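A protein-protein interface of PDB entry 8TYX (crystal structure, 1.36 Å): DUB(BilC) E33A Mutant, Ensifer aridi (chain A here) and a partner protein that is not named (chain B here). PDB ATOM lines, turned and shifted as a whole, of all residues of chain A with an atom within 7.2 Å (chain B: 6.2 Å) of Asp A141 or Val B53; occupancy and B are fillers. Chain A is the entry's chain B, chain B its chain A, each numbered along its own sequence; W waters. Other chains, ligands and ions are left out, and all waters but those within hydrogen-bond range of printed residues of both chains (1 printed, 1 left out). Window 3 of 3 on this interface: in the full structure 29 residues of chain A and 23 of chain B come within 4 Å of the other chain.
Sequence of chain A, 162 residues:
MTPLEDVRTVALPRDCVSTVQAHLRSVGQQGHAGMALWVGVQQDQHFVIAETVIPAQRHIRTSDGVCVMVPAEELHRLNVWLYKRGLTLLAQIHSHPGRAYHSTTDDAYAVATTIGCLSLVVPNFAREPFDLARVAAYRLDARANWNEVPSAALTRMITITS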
ATOM      1  N   GLU A   5      20.583  -2.729  10.109  1.00  0.00           N
ATOM      2  CA  GLU A   5      20.077  -1.687   9.223  1.00  0.00           C
ATOM      3  C   GLU A   5      20.866  -0.388   9.311  1.00  0.00           C
ATOM      4  O   GLU A   5      20.946   0.355   8.326  1.00  0.00           O
ATOM      5  CB  GLU A   5      18.604  -1.409   9.617  1.00  0.00           C
ATOM      6  CG  GLU A   5      17.870  -0.400   8.781  1.00  0.00           C
ATOM      7  CD  GLU A   5      16.401  -0.246   9.132  1.00  0.00           C
ATOM      8  OE1 GLU A   5      15.976  -0.662  10.223  1.00  0.00           O
ATOM      9  OE2 GLU A   5      15.646   0.299   8.303  1.00  0.00           O
ATOM     10  N   THR A 113      18.879 -12.585   5.306  1.00  0.00           N
ATOM     11  CA  THR A 113      17.449 -12.291   5.481  1.00  0.00           C
ATOM     12  C   THR A 113      17.149 -11.119   6.406  1.00  0.00           C
ATOM     13  O   THR A 113      15.973 -10.743   6.518  1.00  0.00           O
ATOM     14  CB  THR A 113      16.738 -13.527   6.025  1.00  0.00           C
ATOM     15  OG1 THR A 113      17.408 -13.950   7.208  1.00  0.00           O
ATOM     16  CG2 THR A 113      16.700 -14.687   5.052  1.00  0.00           C
ATOM     17  N   THR A 114      18.159 -10.542   7.047  1.00  0.00           N
ATOM     18  CA  THR A 114      17.989  -9.515   8.065  1.00  0.00           C
ATOM     19  C   THR A 114      17.857  -8.137   7.412  1.00  0.00           C
ATOM     20  O   THR A 114      18.565  -7.831   6.453  1.00  0.00           O
ATOM     21  CB  THR A 114      19.197  -9.500   9.000  1.00  0.00           C
ATOM     22  OG1 THR A 114      19.561 -10.847   9.306  1.00  0.00           O
ATOM     23  CG2 THR A 114      18.882  -8.761  10.303  1.00  0.00           C
ATOM     24  N   ILE A 115      16.929  -7.310   7.934  1.00  0.00           N
ATOM     25  CA  ILE A 115      16.850  -5.925   7.492  1.00  0.00           C
ATOM     26  C   ILE A 115      18.253  -5.327   7.549  1.00  0.00           C
ATOM     27  O   ILE A 115      18.936  -5.426   8.578  1.00  0.00           O
ATOM     28  CB  ILE A 115      15.873  -5.119   8.360  1.00  0.00           C
ATOM     29  CG1 ILE A 115      14.467  -5.714   8.309  1.00  0.00           C
ATOM     30  CG2 ILE A 115      15.849  -3.652   7.900  1.00  0.00           C
ATOM     31  CD1 ILE A 115      13.545  -5.084   9.329  1.00  0.00           C
ATOM     32  N   GLY A 116      18.692  -4.699   6.446  1.00  0.00           N
ATOM     33  CA  GLY A 116      20.040  -4.163   6.367  1.00  0.00           C
ATOM     34  C   GLY A 116      21.048  -5.041   5.661  1.00  0.00           C
ATOM     35  O   GLY A 116      22.147  -4.550   5.330  1.00  0.00           O
ATOM     36  N   CYS A 117      20.731  -6.318   5.442  1.00  0.00           N
ATOM     37  CA  CYS A 117      21.664  -7.161   4.701  1.00  0.00           C
ATOM     38  C   CYS A 117      21.837  -6.691   3.260  1.00  0.00           C
ATOM     39  O   CYS A 117      20.973  -6.012   2.711  1.00  0.00           O
ATOM     40  CB  CYS A 117      21.134  -8.605   4.648  1.00  0.00           C
ATOM     41  SG  CYS A 117      21.381  -9.551   6.194  1.00  0.00           S
ATOM     42  N   ARG A 139      20.074  -3.744  -1.001  1.00  0.00           N
ATOM     43  CA  ARG A 139      19.994  -3.781   0.443  1.00  0.00           C
ATOM     44  C   ARG A 139      18.536  -3.971   0.859  1.00  0.00           C
ATOM     45  O   ARG A 139      17.628  -3.380   0.265  1.00  0.00           O
ATOM     46  CB  ARG A 139      20.576  -2.509   1.072  1.00  0.00           C
ATOM     47  CG  ARG A 139      20.823  -2.649   2.553  1.00  0.00           C
ATOM     48  CD  ARG A 139      21.655  -1.495   3.054  1.00  0.00           C
ATOM     49  NE  ARG A 139      22.240  -1.808   4.352  1.00  0.00           N
ATOM     50  CZ  ARG A 139      22.906  -0.937   5.090  1.00  0.00           C
ATOM     51  NH1 ARG A 139      23.102   0.304   4.678  1.00  0.00           N
ATOM     52  NH2 ARG A 139      23.369  -1.316   6.279  1.00  0.00           N
ATOM     53  N   LEU A 140      18.325  -4.808   1.875  1.00  0.00           N
ATOM     54  CA  LEU A 140      16.989  -5.190   2.293  1.00  0.00           C
ATOM     55  C   LEU A 140      16.407  -4.152   3.262  1.00  0.00           C
ATOM     56  O   LEU A 140      16.996  -3.868   4.318  1.00  0.00           O
ATOM     57  CB  LEU A 140      17.054  -6.551   3.004  1.00  0.00           C
ATOM     58  CG  LEU A 140      15.733  -7.181   3.382  1.00  0.00           C
ATOM     59  CD1 LEU A 140      14.946  -7.587   2.149  1.00  0.00           C
ATOM     60  CD2 LEU A 140      15.944  -8.413   4.245  1.00  0.00           C
ATOM     61  N   ASP A 141      15.221  -3.657   2.935  1.00  0.00           N
ATOM     62  CA  ASP A 141      14.520  -2.676   3.752  1.00  0.00           C
ATOM     63  C   ASP A 141      13.551  -3.354   4.730  1.00  0.00           C
ATOM     64  O   ASP A 141      13.368  -4.581   4.749  1.00  0.00           O
ATOM     65  CB  ASP A 141      13.884  -1.551   2.891  1.00  0.00           C
ATOM     66  CG  ASP A 141      12.602  -1.953   2.172  1.00  0.00           C
ATOM     67  OD1 ASP A 141      11.985  -2.971   2.508  1.00  0.00           O
ATOM     68  OD2 ASP A 141      12.175  -1.198   1.259  1.00  0.00           O
ATOM     69  N   ALA A 142      12.921  -2.530   5.569  1.00  0.00           N
ATOM     70  CA  ALA A 142      12.075  -3.049   6.641  1.00  0.00           C
ATOM     71  C   ALA A 142      10.796  -3.694   6.124  1.00  0.00           C
ATOM     72  O   ALA A 142      10.171  -4.486   6.839  1.00  0.00           O
ATOM     73  CB  ALA A 142      11.730  -1.928   7.632  1.00  0.00           C
ATOM     74  N   ARG A 143      10.406  -3.412   4.886  1.00  0.00           N
ATOM     75  CA  ARG A 143       9.230  -4.028   4.279  1.00  0.00           C
ATOM     76  C   ARG A 143       9.611  -5.184   3.355  1.00  0.00           C
ATOM     77  O   ARG A 143       8.808  -5.617   2.520  1.00  0.00           O
ATOM     78  CB  ARG A 143       8.405  -2.971   3.545  1.00  0.00           C
ATOM     79  CG  ARG A 143       7.966  -1.812   4.422  1.00  0.00           C
ATOM     80  CD  ARG A 143       7.099  -2.248   5.576  1.00  0.00           C
ATOM     81  NE  ARG A 143       5.941  -3.033   5.167  1.00  0.00           N
ATOM     82  CZ  ARG A 143       4.786  -2.528   4.754  1.00  0.00           C
ATOM     83  NH1 ARG A 143       4.605  -1.222   4.635  1.00  0.00           N
ATOM     84  NH2 ARG A 143       3.799  -3.356   4.442  1.00  0.00           N
ATOM     85  N   ALA A 144      10.826  -5.701   3.510  1.00  0.00           N
ATOM     86  CA  ALA A 144      11.306  -6.899   2.815  1.00  0.00           C
ATOM     87  C   ALA A 144      11.552  -6.672   1.333  1.00  0.00           C
ATOM     88  O   ALA A 144      11.503  -7.619   0.548  1.00  0.00           O
ATOM     89  CB  ALA A 144      10.411  -8.117   3.057  1.00  0.00           C
ATOM     90  N   ASN A 145      11.882  -5.444   0.936  1.00  0.00           N
ATOM     91  CA  ASN A 145      12.230  -5.142  -0.436  1.00  0.00           C
ATOM     92  C   ASN A 145      13.735  -5.037  -0.583  1.00  0.00           C
ATOM     93  O   ASN A 145      14.405  -4.454   0.270  1.00  0.00           O
ATOM     94  CB  ASN A 145      11.614  -3.798  -0.847  1.00  0.00           C
ATOM     95  CG  ASN A 145      10.119  -3.763  -0.701  1.00  0.00           C
ATOM     96  OD1 ASN A 145       9.401  -4.553  -1.307  1.00  0.00           O
ATOM     97  ND2 ASN A 145       9.647  -2.854   0.105  1.00  0.00           N
ATOM     98  N   TRP A 146      14.252  -5.585  -1.663  1.00  0.00           N
ATOM     99  CA  TRP A 146      15.655  -5.457  -2.021  1.00  0.00           C
ATOM    100  C   TRP A 146      15.802  -4.241  -2.931  1.00  0.00           C
ATOM    101  O   TRP A 146      15.369  -4.264  -4.083  1.00  0.00           O
ATOM    102  CB  TRP A 146      16.148  -6.736  -2.709  1.00  0.00           C
ATOM    103  CG  TRP A 146      16.326  -7.900  -1.772  1.00  0.00           C
ATOM    104  CD1 TRP A 146      15.472  -8.965  -1.578  1.00  0.00           C
ATOM    105  CD2 TRP A 146      17.433  -8.118  -0.880  1.00  0.00           C
ATOM    106  NE1 TRP A 146      15.994  -9.820  -0.634  1.00  0.00           N
ATOM    107  CE2 TRP A 146      17.194  -9.321  -0.189  1.00  0.00           C
ATOM    108  CE3 TRP A 146      18.597  -7.398  -0.587  1.00  0.00           C
ATOM    109  CZ2 TRP A 146      18.075  -9.807   0.772  1.00  0.00           C
ATOM    110  CZ3 TRP A 146      19.459  -7.873   0.353  1.00  0.00           C
ATOM    111  CH2 TRP A 146      19.212  -9.069   1.026  1.00  0.00           C
ATOM    112  N   ASN A 147      16.382  -3.163  -2.423  1.00  0.00           N
ATOM    113  CA  ASN A 147      16.506  -1.914  -3.170  1.00  0.00           C
ATOM    114  C   ASN A 147      17.954  -1.690  -3.583  1.00  0.00           C
ATOM    115  O   ASN A 147      18.888  -1.902  -2.797  1.00  0.00           O
ATOM    116  CB  ASN A 147      16.062  -0.732  -2.315  1.00  0.00           C
ATOM    117  CG  ASN A 147      14.634  -0.876  -1.845  1.00  0.00           C
ATOM    118  OD1 ASN A 147      13.716  -1.190  -2.609  1.00  0.00           O
ATOM    119  ND2 ASN A 147      14.432  -0.623  -0.571  1.00  0.00           N
ATOM    120  N   LEU B  47      11.282 -14.242  14.493  1.00  0.00           N
ATOM    121  CA  LEU B  47      11.656 -13.568  13.256  1.00  0.00           C
ATOM    122  C   LEU B  47      11.475 -12.065  13.383  1.00  0.00           C
ATOM    123  O   LEU B  47      12.309 -11.297  12.888  1.00  0.00           O
ATOM    124  CB  LEU B  47      10.843 -14.135  12.098  1.00  0.00           C
ATOM    125  CG  LEU B  47      11.178 -15.584  11.745  1.00  0.00           C
ATOM    126  CD1 LEU B  47      10.166 -16.121  10.763  1.00  0.00           C
ATOM    127  CD2 LEU B  47      12.594 -15.712  11.189  1.00  0.00           C
ATOM    128  N   GLU B  48      10.374 -11.621  14.011  1.00  0.00           N
ATOM    129  CA  GLU B  48      10.182 -10.180  14.187  1.00  0.00           C
ATOM    130  C   GLU B  48      11.253  -9.599  15.102  1.00  0.00           C
ATOM    131  O   GLU B  48      11.811  -8.532  14.814  1.00  0.00           O
ATOM    132  CB  GLU B  48       8.781  -9.930  14.756  1.00  0.00           C
ATOM    133  CG  GLU B  48       8.297  -8.510  14.665  1.00  0.00           C
ATOM    134  CD  GLU B  48       6.772  -8.425  14.681  1.00  0.00           C
ATOM    135  OE1 GLU B  48       6.104  -9.486  14.633  1.00  0.00           O
ATOM    136  OE2 GLU B  48       6.247  -7.295  14.732  1.00  0.00           O
ATOM    137  N   GLN B  51      14.520  -9.192  13.210  1.00  0.00           N
ATOM    138  CA  GLN B  51      14.451  -8.424  11.969  1.00  0.00           C
ATOM    139  C   GLN B  51      14.727  -9.294  10.730  1.00  0.00           C
ATOM    140  O   GLN B  51      15.238  -8.809   9.713  1.00  0.00           O
ATOM    141  CB  GLN B  51      15.356  -7.191  11.970  1.00  0.00           C
ATOM    142  CG  GLN B  51      14.993  -6.116  12.997  1.00  0.00           C
ATOM    143  CD  GLN B  51      15.340  -6.487  14.410  1.00  0.00           C
ATOM    144  OE1 GLN B  51      16.446  -6.929  14.693  1.00  0.00           O
ATOM    145  NE2 GLN B  51      14.383  -6.276  15.328  1.00  0.00           N
ATOM    146  N   ASN B  52      14.358 -10.571  10.784  1.00  0.00           N
ATOM    147  CA  ASN B  52      14.542 -11.475   9.644  1.00  0.00           C
ATOM    148  C   ASN B  52      13.250 -11.512   8.840  1.00  0.00           C
ATOM    149  O   ASN B  52      12.291 -12.200   9.198  1.00  0.00           O
ATOM    150  CB  ASN B  52      15.034 -12.825  10.123  1.00  0.00           C
ATOM    151  CG  ASN B  52      16.498 -12.786  10.449  1.00  0.00           C
ATOM    152  OD1 ASN B  52      17.331 -12.595   9.556  1.00  0.00           O
ATOM    153  ND2 ASN B  52      16.824 -12.882  11.732  1.00  0.00           N
ATOM    154  N   VAL B  53      13.246 -10.753   7.751  1.00  0.00           N
ATOM    155  CA  VAL B  53      12.042 -10.503   6.970  1.00  0.00           C
ATOM    156  C   VAL B  53      12.138 -10.936   5.512  1.00  0.00           C
ATOM    157  O   VAL B  53      11.123 -10.895   4.813  1.00  0.00           O
ATOM    158  CB  VAL B  53      11.637  -9.016   7.031  1.00  0.00           C
ATOM    159  CG1 VAL B  53      11.472  -8.565   8.445  1.00  0.00           C
ATOM    160  CG2 VAL B  53      12.618  -8.106   6.278  1.00  0.00           C
ATOM    161  N   ALA B  54      13.307 -11.336   4.999  1.00  0.00           N
ATOM    162  CA  ALA B  54      13.419 -11.479   3.553  1.00  0.00           C
ATOM    163  C   ALA B  54      12.594 -12.644   3.021  1.00  0.00           C
ATOM    164  O   ALA B  54      12.298 -12.652   1.817  1.00  0.00           O
ATOM    165  CB  ALA B  54      14.882 -11.699   3.146  1.00  0.00           C
ATOM    166  N   GLN B  55      12.279 -13.634   3.854  1.00  0.00           N
ATOM    167  CA  GLN B  55      11.322 -14.671   3.516  1.00  0.00           C
ATOM    168  C   GLN B  55      10.309 -14.742   4.647  1.00  0.00           C
ATOM    169  O   GLN B  55      10.671 -14.519   5.818  1.00  0.00           O
ATOM    170  CB  GLN B  55      12.002 -16.032   3.339  1.00  0.00           C
ATOM    171  CG  GLN B  55      12.975 -16.073   2.171  1.00  0.00           C
ATOM    172  CD  GLN B  55      13.378 -17.492   1.787  1.00  0.00           C
ATOM    173  OE1 GLN B  55      12.533 -18.392   1.731  1.00  0.00           O
ATOM    174  NE2 GLN B  55      14.653 -17.705   1.523  1.00  0.00           N
ATOM    175  N   PRO B  56       9.042 -15.005   4.336  1.00  0.00           N
ATOM    176  CA  PRO B  56       7.981 -14.943   5.369  1.00  0.00           C
ATOM    177  C   PRO B  56       8.069 -16.116   6.327  1.00  0.00           C
ATOM    178  O   PRO B  56       8.784 -17.108   6.074  1.00  0.00           O
ATOM    179  CB  PRO B  56       6.690 -15.007   4.538  1.00  0.00           C
ATOM    180  CG  PRO B  56       7.084 -15.772   3.320  1.00  0.00           C
ATOM    181  CD  PRO B  56       8.495 -15.348   3.008  1.00  0.00           C
ATOM    182  N   TRP B  60      10.429 -20.936   7.121  1.00  0.00           N
ATOM    183  CA  TRP B  60      11.437 -21.260   8.118  1.00  0.00           C
ATOM    184  C   TRP B  60      10.980 -22.468   8.927  1.00  0.00           C
ATOM    185  O   TRP B  60       9.778 -22.711   9.104  1.00  0.00           O
ATOM    186  CB  TRP B  60      11.650 -20.082   9.091  1.00  0.00           C
ATOM    187  CG  TRP B  60      12.068 -18.778   8.477  1.00  0.00           C
ATOM    188  CD1 TRP B  60      11.278 -17.934   7.764  1.00  0.00           C
ATOM    189  CD2 TRP B  60      13.356 -18.155   8.567  1.00  0.00           C
ATOM    190  NE1 TRP B  60      11.997 -16.822   7.398  1.00  0.00           N
ATOM    191  CE2 TRP B  60      13.278 -16.946   7.874  1.00  0.00           C
ATOM    192  CE3 TRP B  60      14.563 -18.513   9.160  1.00  0.00           C
ATOM    193  CZ2 TRP B  60      14.362 -16.077   7.777  1.00  0.00           C
ATOM    194  CZ3 TRP B  60      15.647 -17.658   9.042  1.00  0.00           C
ATOM    195  CH2 TRP B  60      15.550 -16.468   8.351  1.00  0.00           C
HETATM  196  O   HOH W   1      14.339 -12.591  -0.197  1.00  0.00           O
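The side-chain amide nitrogen of Asn A147 lies within hydrogen-bond range of the side-chain carboxylate of Asp A141 (3.0 Å). OD1 of Asp A141 is in hydrogen-bond range of N of Asn A145, 2.9 Å away. OD1 of Asp A141 lies within hydrogen-bond range of N of Arg A143 (2.9 Å). The backbone carbonyl oxygen of Leu B47 sits at hydrogen-bond distance from the backbone NH of Asn B52. NE2 of Gln B51 lies within hydrogen-bond range of O of Glu B48, at 3.5 Å. O of Leu A140 is in hydrogen-bond range of N of Gly A116.
Gln B51 touches Thr A113. Trp B60 touches Thr A113 (CH2 to OG1, 3.3 Å). CA of Thr A114 touches O of Gln B51 (3.3 Å). Ile A115 touches Val B53 (CG1 to CG2, 3.6 Å). Val B53 touches Leu A140 (CG2 to CD2, 3.9 Å). Leu A140 touches Ala B54. Val B53 touches Asp A141. Val B53 touches Ala A144.
Water W1 bridges the backbone carbonyl oxygen of Ala B54 and the indole nitrogen of Trp A146.
Along chain A the printed residues that touch a printed residue of chain B span positions 113 to 144. Among the printed residues, no Asp or Glu carboxylate lies within 4 Å of a Lys or Arg side-chain nitrogen of the other chain.
Asp A141 touches just one residue of chain B: Val B53. Of chain A, only Thr A113, Ile A115, Leu A140, Asp A141 and Ala A144 come within 4 Å of Val B53. Of the printed residues of chain B, Thr A114 touches Gln B51 and Asn B52. Printed residues of chain A within 4 Å of Asn B52: Thr A113 (2.7 Å) and Thr A114 (2.8 Å). Of the printed residues of chain B, Thr A113 touches Gln B51, Asn B52, Val B53, Ala B54 and Trp B60. The nearest printed residue of chain B that does not touch Asp A141 is Ala B54 (6.8 Å).
The backbone NH of Val B53 sits at hydrogen-bond distance from the backbone carbonyl oxygen of Thr A113. The side-chain amide oxygen of Asn B52 is in hydrogen-bond range of the side-chain hydroxyl of Thr A114, at 2.8 Å. The side-chain amide oxygen (OD1) of Asn B52 is in hydrogen-bond range of the side-chain hydroxyl (OG1) of Thr A113. O of Thr A113 lies within hydrogen-bond range of N of Ala B54, at 3.1 Å. The backbone NH of Ile A115 sits at hydrogen-bond distance from the backbone carbonyl oxygen of Gln B51, at 2.9 Å.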
